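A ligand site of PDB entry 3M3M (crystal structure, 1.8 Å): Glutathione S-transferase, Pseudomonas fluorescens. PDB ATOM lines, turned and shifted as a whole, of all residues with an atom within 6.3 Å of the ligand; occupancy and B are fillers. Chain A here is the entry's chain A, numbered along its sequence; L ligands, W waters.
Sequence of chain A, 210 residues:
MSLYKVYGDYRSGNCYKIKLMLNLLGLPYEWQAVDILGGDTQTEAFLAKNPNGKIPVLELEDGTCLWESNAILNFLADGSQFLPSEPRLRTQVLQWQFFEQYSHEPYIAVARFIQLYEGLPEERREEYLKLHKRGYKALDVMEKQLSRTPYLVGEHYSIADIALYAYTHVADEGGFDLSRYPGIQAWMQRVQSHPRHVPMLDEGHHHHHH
Residues that only touch the ligand: Ile 36 (3.5 Å), Gly 53 (3.5 Å) and Pro 56 (3.6 Å). Hydrophobic or aromatic side chains within 4 Å of the ligand: Ile 36, Ile 55 and Pro 56. The nearest printed residue that does not touch the ligand is Lys 17 (4.4 Å).
The side-chain carboxylate (OE1) of Glu 68 lies within salt-bridge range of a nitrogen (N1) of the ligand (2.7 Å). The side-chain amide nitrogen (NE2) of Gln 101 sits close to a nitrogen (N1) of the ligand, at 2.7 Å. The backbone NH (N) of Ser 69 sits at hydrogen-bond distance from an oxygen (O1) of the ligand (2.8 Å). The side-chain hydroxyl (OG) of Ser 69 sits at hydrogen-bond distance from an oxygen (O2) of the ligand (2.7 Å). An oxygen (O4) of the ligand lies within hydrogen-bond range of the backbone NH of Ile 55 (2.8 Å). A nitrogen (N2) of the ligand lies within hydrogen-bond range of the backbone carbonyl oxygen of Ile 55, at 2.8 Å. The side-chain hydroxyl of Ser 12 sits close to a sulfur (S1) of the ligand. The side-chain amino group (NZ) of Lys 54 lies within salt-bridge range of an oxygen (O6) of the ligand (3.0 Å). The side-chain hydroxyl (OH) of Tyr 167 sits close to a sulfur (S1) of the ligand (3.3 Å). O2 of the ligand sits at hydrogen-bond distance from ND2 of Asn 14, 3.4 Å away. The side-chain hydroxyl (OG1) of Thr 41 sits at hydrogen-bond distance from an oxygen (O5) of the ligand (3.4 Å).
Water W4 lies within hydrogen-bond range of the side-chain amino group of Lys 54 (2.6 Å) and an oxygen (O3) of the ligand (2.7 Å). Water W3 lies within hydrogen-bond range of the side-chain carboxylate of Glu 68, a nitrogen (N1) of the ligand and the side-chain amide nitrogen of Asn 52. Water W1 lies within hydrogen-bond range of O1 of the ligand, O of Pro 56 and N of Glu 68. Water W7 lies within hydrogen-bond range of an oxygen (O6) of the ligand (2.8 Å), the backbone carbonyl oxygen (O) of Asn 52 (3.2 Å), the backbone carbonyl oxygen (O) of Gly 53 (3.2 Å) and the side-chain amino group (NZ) of Lys 54 (3.3 Å). Water W2 lies within hydrogen-bond range of OE2 of Glu 105 (2.6 Å) and O3 of the ligand (3.0 Å). Water W5 lies within hydrogen-bond range of OH of Tyr 167 and S1 of the ligand.
OE1 of Glu 100 lies close to OE1 of Gln 101 (3.0 Å). The side-chain hydroxyl (OG) of Ser 69 sits at hydrogen-bond distance from the side-chain amide nitrogen (ND2) of Asn 14 (3.5 Å). The side-chain amino group of Lys 17 is in hydrogen-bond range of the side-chain hydroxyl of Ser 69 (3.1 Å). OG of Ser 12 sits close to N of Asn 14 (3.3 Å). N of Cys 15 sits at hydrogen-bond distance from OG of Ser 12. OD1 of Asn 14 sits at hydrogen-bond distance from OH of Tyr 167. OH of Tyr 167 sits at hydrogen-bond distance from N of Gly 13. The side-chain amide oxygen (OD1) of Asn 14 lies close to the side-chain carboxylate (OE2) of Glu 105.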
ATOM      1  N   SER A  12     -18.575 -26.904 -11.830  1.00  0.00           N
ATOM      2  CA  SER A  12     -17.223 -27.074 -11.274  1.00  0.00           C
ATOM      3  C   SER A  12     -17.087 -28.476 -10.674  1.00  0.00           C
ATOM      4  O   SER A  12     -17.930 -28.834  -9.847  1.00  0.00           O
ATOM      5  CB  SER A  12     -17.061 -26.066 -10.134  1.00  0.00           C
ATOM      6  OG  SER A  12     -16.001 -26.478  -9.200  1.00  0.00           O
ATOM      7  N   GLY A  13     -16.078 -29.231 -11.104  1.00  0.00           N
ATOM      8  CA  GLY A  13     -15.855 -30.556 -10.596  1.00  0.00           C
ATOM      9  C   GLY A  13     -15.668 -30.509  -9.087  1.00  0.00           C
ATOM     10  O   GLY A  13     -16.149 -31.397  -8.378  1.00  0.00           O
ATOM     11  N   ASN A  14     -14.935 -29.505  -8.578  1.00  0.00           N
ATOM     12  CA  ASN A  14     -14.725 -29.416  -7.123  1.00  0.00           C
ATOM     13  C   ASN A  14     -16.043 -29.257  -6.350  1.00  0.00           C
ATOM     14  O   ASN A  14     -16.221 -29.810  -5.269  1.00  0.00           O
ATOM     15  CB  ASN A  14     -13.757 -28.282  -6.775  1.00  0.00           C
ATOM     16  CG  ASN A  14     -12.370 -28.585  -7.329  1.00  0.00           C
ATOM     17  OD1 ASN A  14     -11.790 -27.749  -8.085  1.00  0.00           O
ATOM     18  ND2 ASN A  14     -11.835 -29.764  -6.965  1.00  0.00           N
ATOM     19  N   CYS A  15     -17.009 -28.546  -6.947  1.00  0.00           N
ATOM     20  CA  CYS A  15     -18.325 -28.389  -6.323  1.00  0.00           C
ATOM     21  C   CYS A  15     -19.217 -29.623  -6.519  1.00  0.00           C
ATOM     22  O   CYS A  15     -20.016 -29.971  -5.607  1.00  0.00           O
ATOM     23  CB  CYS A  15     -19.024 -27.155  -6.973  1.00  0.00           C
ATOM     24  SG  CYS A  15     -18.144 -25.602  -6.581  1.00  0.00           S
ATOM     25  N   LYS A  17     -18.211 -32.658  -6.383  1.00  0.00           N
ATOM     26  CA  LYS A  17     -17.902 -33.547  -5.289  1.00  0.00           C
ATOM     27  C   LYS A  17     -18.824 -33.372  -4.103  1.00  0.00           C
ATOM     28  O   LYS A  17     -19.234 -34.401  -3.514  1.00  0.00           O
ATOM     29  CB  LYS A  17     -16.475 -33.210  -4.697  1.00  0.00           C
ATOM     30  CG  LYS A  17     -15.335 -33.483  -5.667  1.00  0.00           C
ATOM     31  CD  LYS A  17     -14.077 -32.785  -5.161  1.00  0.00           C
ATOM     32  CE  LYS A  17     -12.957 -32.948  -6.190  1.00  0.00           C
ATOM     33  NZ  LYS A  17     -11.666 -32.277  -5.730  1.00  0.00           N
ATOM     34  N   ILE A  36     -18.107 -17.300 -11.084  1.00  0.00           N
ATOM     35  CA  ILE A  36     -16.727 -16.871 -10.862  1.00  0.00           C
ATOM     36  C   ILE A  36     -16.400 -15.836 -11.958  1.00  0.00           C
ATOM     37  O   ILE A  36     -15.802 -14.809 -11.643  1.00  0.00           O
ATOM     38  CB  ILE A  36     -15.777 -18.056 -11.051  1.00  0.00           C
ATOM     39  CG1 ILE A  36     -15.908 -19.008  -9.856  1.00  0.00           C
ATOM     40  CG2 ILE A  36     -14.336 -17.500 -11.280  1.00  0.00           C
ATOM     41  CD1 ILE A  36     -15.323 -20.387 -10.187  1.00  0.00           C
ATOM     42  N   THR A  41     -16.531 -14.447  -6.542  1.00  0.00           N
ATOM     43  CA  THR A  41     -15.562 -14.985  -5.563  1.00  0.00           C
ATOM     44  C   THR A  41     -14.532 -13.937  -5.133  1.00  0.00           C
ATOM     45  O   THR A  41     -13.644 -14.251  -4.333  1.00  0.00           O
ATOM     46  CB  THR A  41     -14.762 -16.226  -6.113  1.00  0.00           C
ATOM     47  OG1 THR A  41     -14.053 -15.904  -7.335  1.00  0.00           O
ATOM     48  CG2 THR A  41     -15.704 -17.437  -6.293  1.00  0.00           C
ATOM     49  N   GLN A  42     -14.651 -12.730  -5.689  1.00  0.00           N
ATOM     50  CA  GLN A  42     -13.680 -11.650  -5.371  1.00  0.00           C
ATOM     51  C   GLN A  42     -14.286 -10.568  -4.512  1.00  0.00           C
ATOM     52  O   GLN A  42     -13.597  -9.566  -4.233  1.00  0.00           O
ATOM     53  CB  GLN A  42     -13.159 -10.984  -6.653  1.00  0.00           C
ATOM     54  CG  GLN A  42     -12.500 -11.967  -7.651  1.00  0.00           C
ATOM     55  CD  GLN A  42     -11.945 -11.220  -8.889  1.00  0.00           C
ATOM     56  OE1 GLN A  42     -12.677 -10.467  -9.551  1.00  0.00           O
ATOM     57  NE2 GLN A  42     -10.642 -11.375  -9.168  1.00  0.00           N
ATOM     58  N   PHE A  46     -17.685 -12.655  -0.063  1.00  0.00           N
ATOM     59  CA  PHE A  46     -17.247 -14.028  -0.352  1.00  0.00           C
ATOM     60  C   PHE A  46     -15.912 -14.340   0.438  1.00  0.00           C
ATOM     61  O   PHE A  46     -15.766 -15.412   1.014  1.00  0.00           O
ATOM     62  CB  PHE A  46     -17.041 -14.281  -1.822  1.00  0.00           C
ATOM     63  CG  PHE A  46     -16.814 -15.776  -2.082  1.00  0.00           C
ATOM     64  CD1 PHE A  46     -17.901 -16.653  -2.117  1.00  0.00           C
ATOM     65  CD2 PHE A  46     -15.513 -16.272  -2.104  1.00  0.00           C
ATOM     66  CE1 PHE A  46     -17.641 -18.072  -2.344  1.00  0.00           C
ATOM     67  CE2 PHE A  46     -15.215 -17.615  -2.324  1.00  0.00           C
ATOM     68  CZ  PHE A  46     -16.291 -18.536  -2.457  1.00  0.00           C
ATOM     69  N   ASN A  52      -9.361 -17.689   0.533  1.00  0.00           N
ATOM     70  CA  ASN A  52      -8.619 -18.134  -0.626  1.00  0.00           C
ATOM     71  C   ASN A  52      -9.424 -17.852  -1.914  1.00  0.00           C
ATOM     72  O   ASN A  52      -8.865 -17.977  -2.996  1.00  0.00           O
ATOM     73  CB  ASN A  52      -8.301 -19.657  -0.503  1.00  0.00           C
ATOM     74  CG  ASN A  52      -7.241 -20.112  -1.474  1.00  0.00           C
ATOM     75  OD1 ASN A  52      -6.228 -19.449  -1.621  1.00  0.00           O
ATOM     76  ND2 ASN A  52      -7.418 -21.324  -2.083  1.00  0.00           N
ATOM     77  N   GLY A  53     -10.695 -17.411  -1.797  1.00  0.00           N
ATOM     78  CA  GLY A  53     -11.394 -16.897  -3.001  1.00  0.00           C
ATOM     79  C   GLY A  53     -11.858 -18.019  -3.957  1.00  0.00           C
ATOM     80  O   GLY A  53     -11.971 -17.793  -5.162  1.00  0.00           O
ATOM     81  N   LYS A  54     -12.108 -19.204  -3.394  1.00  0.00           N
ATOM     82  CA  LYS A  54     -12.580 -20.358  -4.233  1.00  0.00           C
ATOM     83  C   LYS A  54     -13.850 -20.992  -3.762  1.00  0.00           C
ATOM     84  O   LYS A  54     -14.156 -21.003  -2.559  1.00  0.00           O
ATOM     85  CB  LYS A  54     -11.511 -21.476  -4.260  1.00  0.00           C
ATOM     86  CG  LYS A  54     -10.190 -20.912  -5.079  1.00  0.00           C
ATOM     87  CD  LYS A  54      -9.145 -21.967  -5.213  1.00  0.00           C
ATOM     88  CE  LYS A  54      -7.792 -21.354  -5.736  1.00  0.00           C
ATOM     89  NZ  LYS A  54      -7.805 -20.372  -6.838  1.00  0.00           N
ATOM     90  N   ILE A  55     -14.565 -21.603  -4.711  1.00  0.00           N
ATOM     91  CA  ILE A  55     -15.698 -22.481  -4.365  1.00  0.00           C
ATOM     92  C   ILE A  55     -15.144 -23.930  -4.558  1.00  0.00           C
ATOM     93  O   ILE A  55     -14.222 -24.181  -5.315  1.00  0.00           O
ATOM     94  CB  ILE A  55     -16.904 -22.227  -5.297  1.00  0.00           C
ATOM     95  CG1 ILE A  55     -16.450 -22.177  -6.744  1.00  0.00           C
ATOM     96  CG2 ILE A  55     -17.601 -20.914  -4.712  1.00  0.00           C
ATOM     97  CD1 ILE A  55     -17.605 -21.888  -7.721  1.00  0.00           C
ATOM     98  N   PRO A  56     -15.711 -24.889  -3.823  1.00  0.00           N
ATOM     99  CA  PRO A  56     -16.927 -24.773  -2.959  1.00  0.00           C
ATOM    100  C   PRO A  56     -16.568 -24.272  -1.541  1.00  0.00           C
ATOM    101  O   PRO A  56     -15.386 -24.364  -1.069  1.00  0.00           O
ATOM    102  CB  PRO A  56     -17.456 -26.208  -2.944  1.00  0.00           C
ATOM    103  CG  PRO A  56     -16.120 -27.016  -2.955  1.00  0.00           C
ATOM    104  CD  PRO A  56     -15.336 -26.293  -4.061  1.00  0.00           C
ATOM    105  N   TRP A  67     -13.872 -24.712   3.800  1.00  0.00           N
ATOM    106  CA  TRP A  67     -13.558 -24.692   2.404  1.00  0.00           C
ATOM    107  C   TRP A  67     -12.471 -25.786   2.127  1.00  0.00           C
ATOM    108  O   TRP A  67     -12.064 -26.472   3.085  1.00  0.00           O
ATOM    109  CB  TRP A  67     -13.131 -23.266   1.954  1.00  0.00           C
ATOM    110  CG  TRP A  67     -12.221 -22.505   2.900  1.00  0.00           C
ATOM    111  CD1 TRP A  67     -12.588 -21.663   3.955  1.00  0.00           C
ATOM    112  CD2 TRP A  67     -10.787 -22.377   2.790  1.00  0.00           C
ATOM    113  NE1 TRP A  67     -11.458 -21.092   4.532  1.00  0.00           N
ATOM    114  CE2 TRP A  67     -10.357 -21.525   3.846  1.00  0.00           C
ATOM    115  CE3 TRP A  67      -9.833 -22.881   1.883  1.00  0.00           C
ATOM    116  CZ2 TRP A  67      -9.024 -21.178   4.017  1.00  0.00           C
ATOM    117  CZ3 TRP A  67      -8.473 -22.575   2.087  1.00  0.00           C
ATOM    118  CH2 TRP A  67      -8.093 -21.773   3.172  1.00  0.00           C
ATOM    119  N   GLU A  68     -12.096 -25.904   0.854  1.00  0.00           N
ATOM    120  CA  GLU A  68     -11.420 -27.013   0.228  1.00  0.00           C
ATOM    121  C   GLU A  68     -12.390 -28.197   0.070  1.00  0.00           C
ATOM    122  O   GLU A  68     -12.747 -28.770   0.971  1.00  0.00           O
ATOM    123  CB  GLU A  68     -10.161 -27.409   0.980  1.00  0.00           C
ATOM    124  CG  GLU A  68      -9.039 -26.388   0.841  1.00  0.00           C
ATOM    125  CD  GLU A  68      -8.535 -26.217  -0.566  1.00  0.00           C
ATOM    126  OE1 GLU A  68      -8.400 -27.186  -1.256  1.00  0.00           O
ATOM    127  OE2 GLU A  68      -8.192 -25.113  -0.855  1.00  0.00           O
ATOM    128  N   SER A  69     -12.721 -28.485  -1.170  1.00  0.00           N
ATOM    129  CA  SER A  69     -13.660 -29.551  -1.474  1.00  0.00           C
ATOM    130  C   SER A  69     -13.249 -30.849  -0.823  1.00  0.00           C
ATOM    131  O   SER A  69     -14.126 -31.540  -0.290  1.00  0.00           O
ATOM    132  CB  SER A  69     -13.755 -29.790  -3.025  1.00  0.00           C
ATOM    133  OG  SER A  69     -12.515 -30.184  -3.601  1.00  0.00           O
ATOM    134  N   ASN A  70     -11.972 -31.183  -0.841  1.00  0.00           N
ATOM    135  CA  ASN A  70     -11.600 -32.487  -0.254  1.00  0.00           C
ATOM    136  C   ASN A  70     -11.695 -32.495   1.290  1.00  0.00           C
ATOM    137  O   ASN A  70     -11.934 -33.561   1.874  1.00  0.00           O
ATOM    138  CB  ASN A  70     -10.234 -32.956  -0.703  1.00  0.00           C
ATOM    139  CG  ASN A  70     -10.222 -33.408  -2.163  1.00  0.00           C
ATOM    140  OD1 ASN A  70     -11.246 -33.500  -2.828  1.00  0.00           O
ATOM    141  ND2 ASN A  70      -9.019 -33.630  -2.691  1.00  0.00           N
ATOM    142  N   ILE A  72     -13.987 -30.689   2.883  1.00  0.00           N
ATOM    143  CA  ILE A  72     -15.468 -30.799   3.053  1.00  0.00           C
ATOM    144  C   ILE A  72     -15.936 -32.255   2.900  1.00  0.00           C
ATOM    145  O   ILE A  72     -16.750 -32.737   3.721  1.00  0.00           O
ATOM    146  CB  ILE A  72     -16.215 -29.840   2.066  1.00  0.00           C
ATOM    147  CG1 ILE A  72     -15.878 -28.360   2.385  1.00  0.00           C
ATOM    148  CG2 ILE A  72     -17.775 -30.150   2.174  1.00  0.00           C
ATOM    149  CD1 ILE A  72     -16.190 -27.476   1.120  1.00  0.00           C
ATOM    150  N   GLU A 100      -5.016 -36.263  -5.922  1.00  0.00           N
ATOM    151  CA  GLU A 100      -5.985 -35.595  -6.860  1.00  0.00           C
ATOM    152  C   GLU A 100      -5.762 -34.056  -6.960  1.00  0.00           C
ATOM    153  O   GLU A 100      -5.756 -33.481  -8.130  1.00  0.00           O
ATOM    154  CB  GLU A 100      -7.438 -35.860  -6.399  1.00  0.00           C
ATOM    155  CG  GLU A 100      -8.475 -35.183  -7.328  1.00  0.00           C
ATOM    156  CD  GLU A 100      -9.012 -33.826  -6.786  1.00  0.00           C
ATOM    157  OE1 GLU A 100      -8.923 -33.573  -5.579  1.00  0.00           O
ATOM    158  OE2 GLU A 100      -9.651 -33.100  -7.553  1.00  0.00           O
ATOM    159  N   GLN A 101      -5.454 -33.414  -5.816  1.00  0.00           N
ATOM    160  CA  GLN A 101      -5.250 -31.971  -5.814  1.00  0.00           C
ATOM    161  C   GLN A 101      -3.855 -31.595  -6.464  1.00  0.00           C
ATOM    162  O   GLN A 101      -3.764 -30.518  -7.071  1.00  0.00           O
ATOM    163  CB  GLN A 101      -5.328 -31.466  -4.343  1.00  0.00           C
ATOM    164  CG  GLN A 101      -6.776 -31.452  -3.842  1.00  0.00           C
ATOM    165  CD  GLN A 101      -7.619 -30.363  -4.544  1.00  0.00           C
ATOM    166  OE1 GLN A 101      -8.696 -30.651  -5.214  1.00  0.00           O
ATOM    167  NE2 GLN A 101      -7.188 -29.132  -4.423  1.00  0.00           N
ATOM    168  N   GLU A 105      -6.087 -32.873 -10.707  1.00  0.00           N
ATOM    169  CA  GLU A 105      -6.942 -31.686 -10.920  1.00  0.00           C
ATOM    170  C   GLU A 105      -6.275 -30.563 -11.805  1.00  0.00           C
ATOM    171  O   GLU A 105      -6.870 -30.083 -12.782  1.00  0.00           O
ATOM    172  CB  GLU A 105      -7.527 -31.166  -9.544  1.00  0.00           C
ATOM    173  CG  GLU A 105      -8.786 -30.332  -9.695  1.00  0.00           C
ATOM    174  CD  GLU A 105      -8.565 -28.888  -9.938  1.00  0.00           C
ATOM    175  OE1 GLU A 105      -7.398 -28.461 -10.293  1.00  0.00           O
ATOM    176  OE2 GLU A 105      -9.570 -28.086  -9.844  1.00  0.00           O
ATOM    177  N   TYR A 167     -13.783 -34.842 -11.728  1.00  0.00           N
ATOM    178  CA  TYR A 167     -13.319 -34.396 -12.987  1.00  0.00           C
ATOM    179  C   TYR A 167     -13.017 -35.589 -13.932  1.00  0.00           C
ATOM    180  O   TYR A 167     -13.022 -35.359 -15.148  1.00  0.00           O
ATOM    181  CB  TYR A 167     -11.989 -33.590 -12.807  1.00  0.00           C
ATOM    182  CG  TYR A 167     -12.337 -32.164 -12.369  1.00  0.00           C
ATOM    183  CD1 TYR A 167     -12.853 -31.237 -13.307  1.00  0.00           C
ATOM    184  CD2 TYR A 167     -12.046 -31.768 -11.068  1.00  0.00           C
ATOM    185  CE1 TYR A 167     -13.161 -29.886 -12.877  1.00  0.00           C
ATOM    186  CE2 TYR A 167     -12.297 -30.427 -10.654  1.00  0.00           C
ATOM    187  CZ  TYR A 167     -12.826 -29.504 -11.565  1.00  0.00           C
ATOM    188  OH  TYR A 167     -13.142 -28.185 -11.095  1.00  0.00           O
HETATM  189  N1  LIG L   1      -8.267 -26.723  -3.885  1.00  0.00           N
HETATM  190  C1  LIG L   1      -9.662 -26.161  -4.051  1.00  0.00           C
HETATM  191  C2  LIG L   1     -10.744 -27.200  -3.765  1.00  0.00           C
HETATM  192  O1  LIG L   1     -11.822 -26.795  -3.233  1.00  0.00           O
HETATM  193  O2  LIG L   1     -10.542 -28.388  -4.122  1.00  0.00           O
HETATM  194  C3  LIG L   1      -9.729 -25.653  -5.528  1.00  0.00           C
HETATM  195  C4  LIG L   1     -11.108 -25.096  -5.724  1.00  0.00           C
HETATM  196  C5  LIG L   1     -11.181 -24.263  -7.017  1.00  0.00           C
HETATM  197  O3  LIG L   1     -10.072 -24.131  -7.847  1.00  0.00           O
HETATM  198  N2  LIG L   1     -12.335 -23.634  -7.378  1.00  0.00           N
HETATM  199  C6  LIG L   1     -12.391 -22.855  -8.616  1.00  0.00           C
HETATM  200  C7  LIG L   1     -12.550 -21.455  -8.223  1.00  0.00           C
HETATM  201  O4  LIG L   1     -13.342 -21.186  -7.188  1.00  0.00           O
HETATM  202  C8  LIG L   1     -13.642 -23.362  -9.394  1.00  0.00           C
HETATM  203  S1  LIG L   1     -13.431 -25.165  -9.890  1.00  0.00           S
HETATM  204  N3  LIG L   1     -11.909 -20.502  -8.867  1.00  0.00           N
HETATM  205  C9  LIG L   1     -12.183 -19.100  -8.481  1.00  0.00           C
HETATM  206  C10 LIG L   1     -10.944 -18.231  -8.479  1.00  0.00           C
HETATM  207  O5  LIG L   1     -11.044 -16.971  -8.551  1.00  0.00           O
HETATM  208  O6  LIG L   1      -9.822 -18.764  -8.357  1.00  0.00           O
HETATM  209  O   HOH W   1     -12.593 -24.515  -1.759  1.00  0.00           O
HETATM  210  O   HOH W   2      -9.799 -25.535 -10.464  1.00  0.00           O
HETATM  211  O   HOH W   3      -7.100 -24.307  -3.096  1.00  0.00           O
HETATM  212  O   HOH W   4      -8.523 -22.073  -8.659  1.00  0.00           O
HETATM  213  O   HOH W   5     -14.200 -26.578 -12.731  1.00  0.00           O
HETATM  214  O   HOH W   6     -10.111 -21.479 -10.929  1.00  0.00           O
HETATM  215  O   HOH W   7      -8.915 -17.329  -6.089  1.00  0.00           O
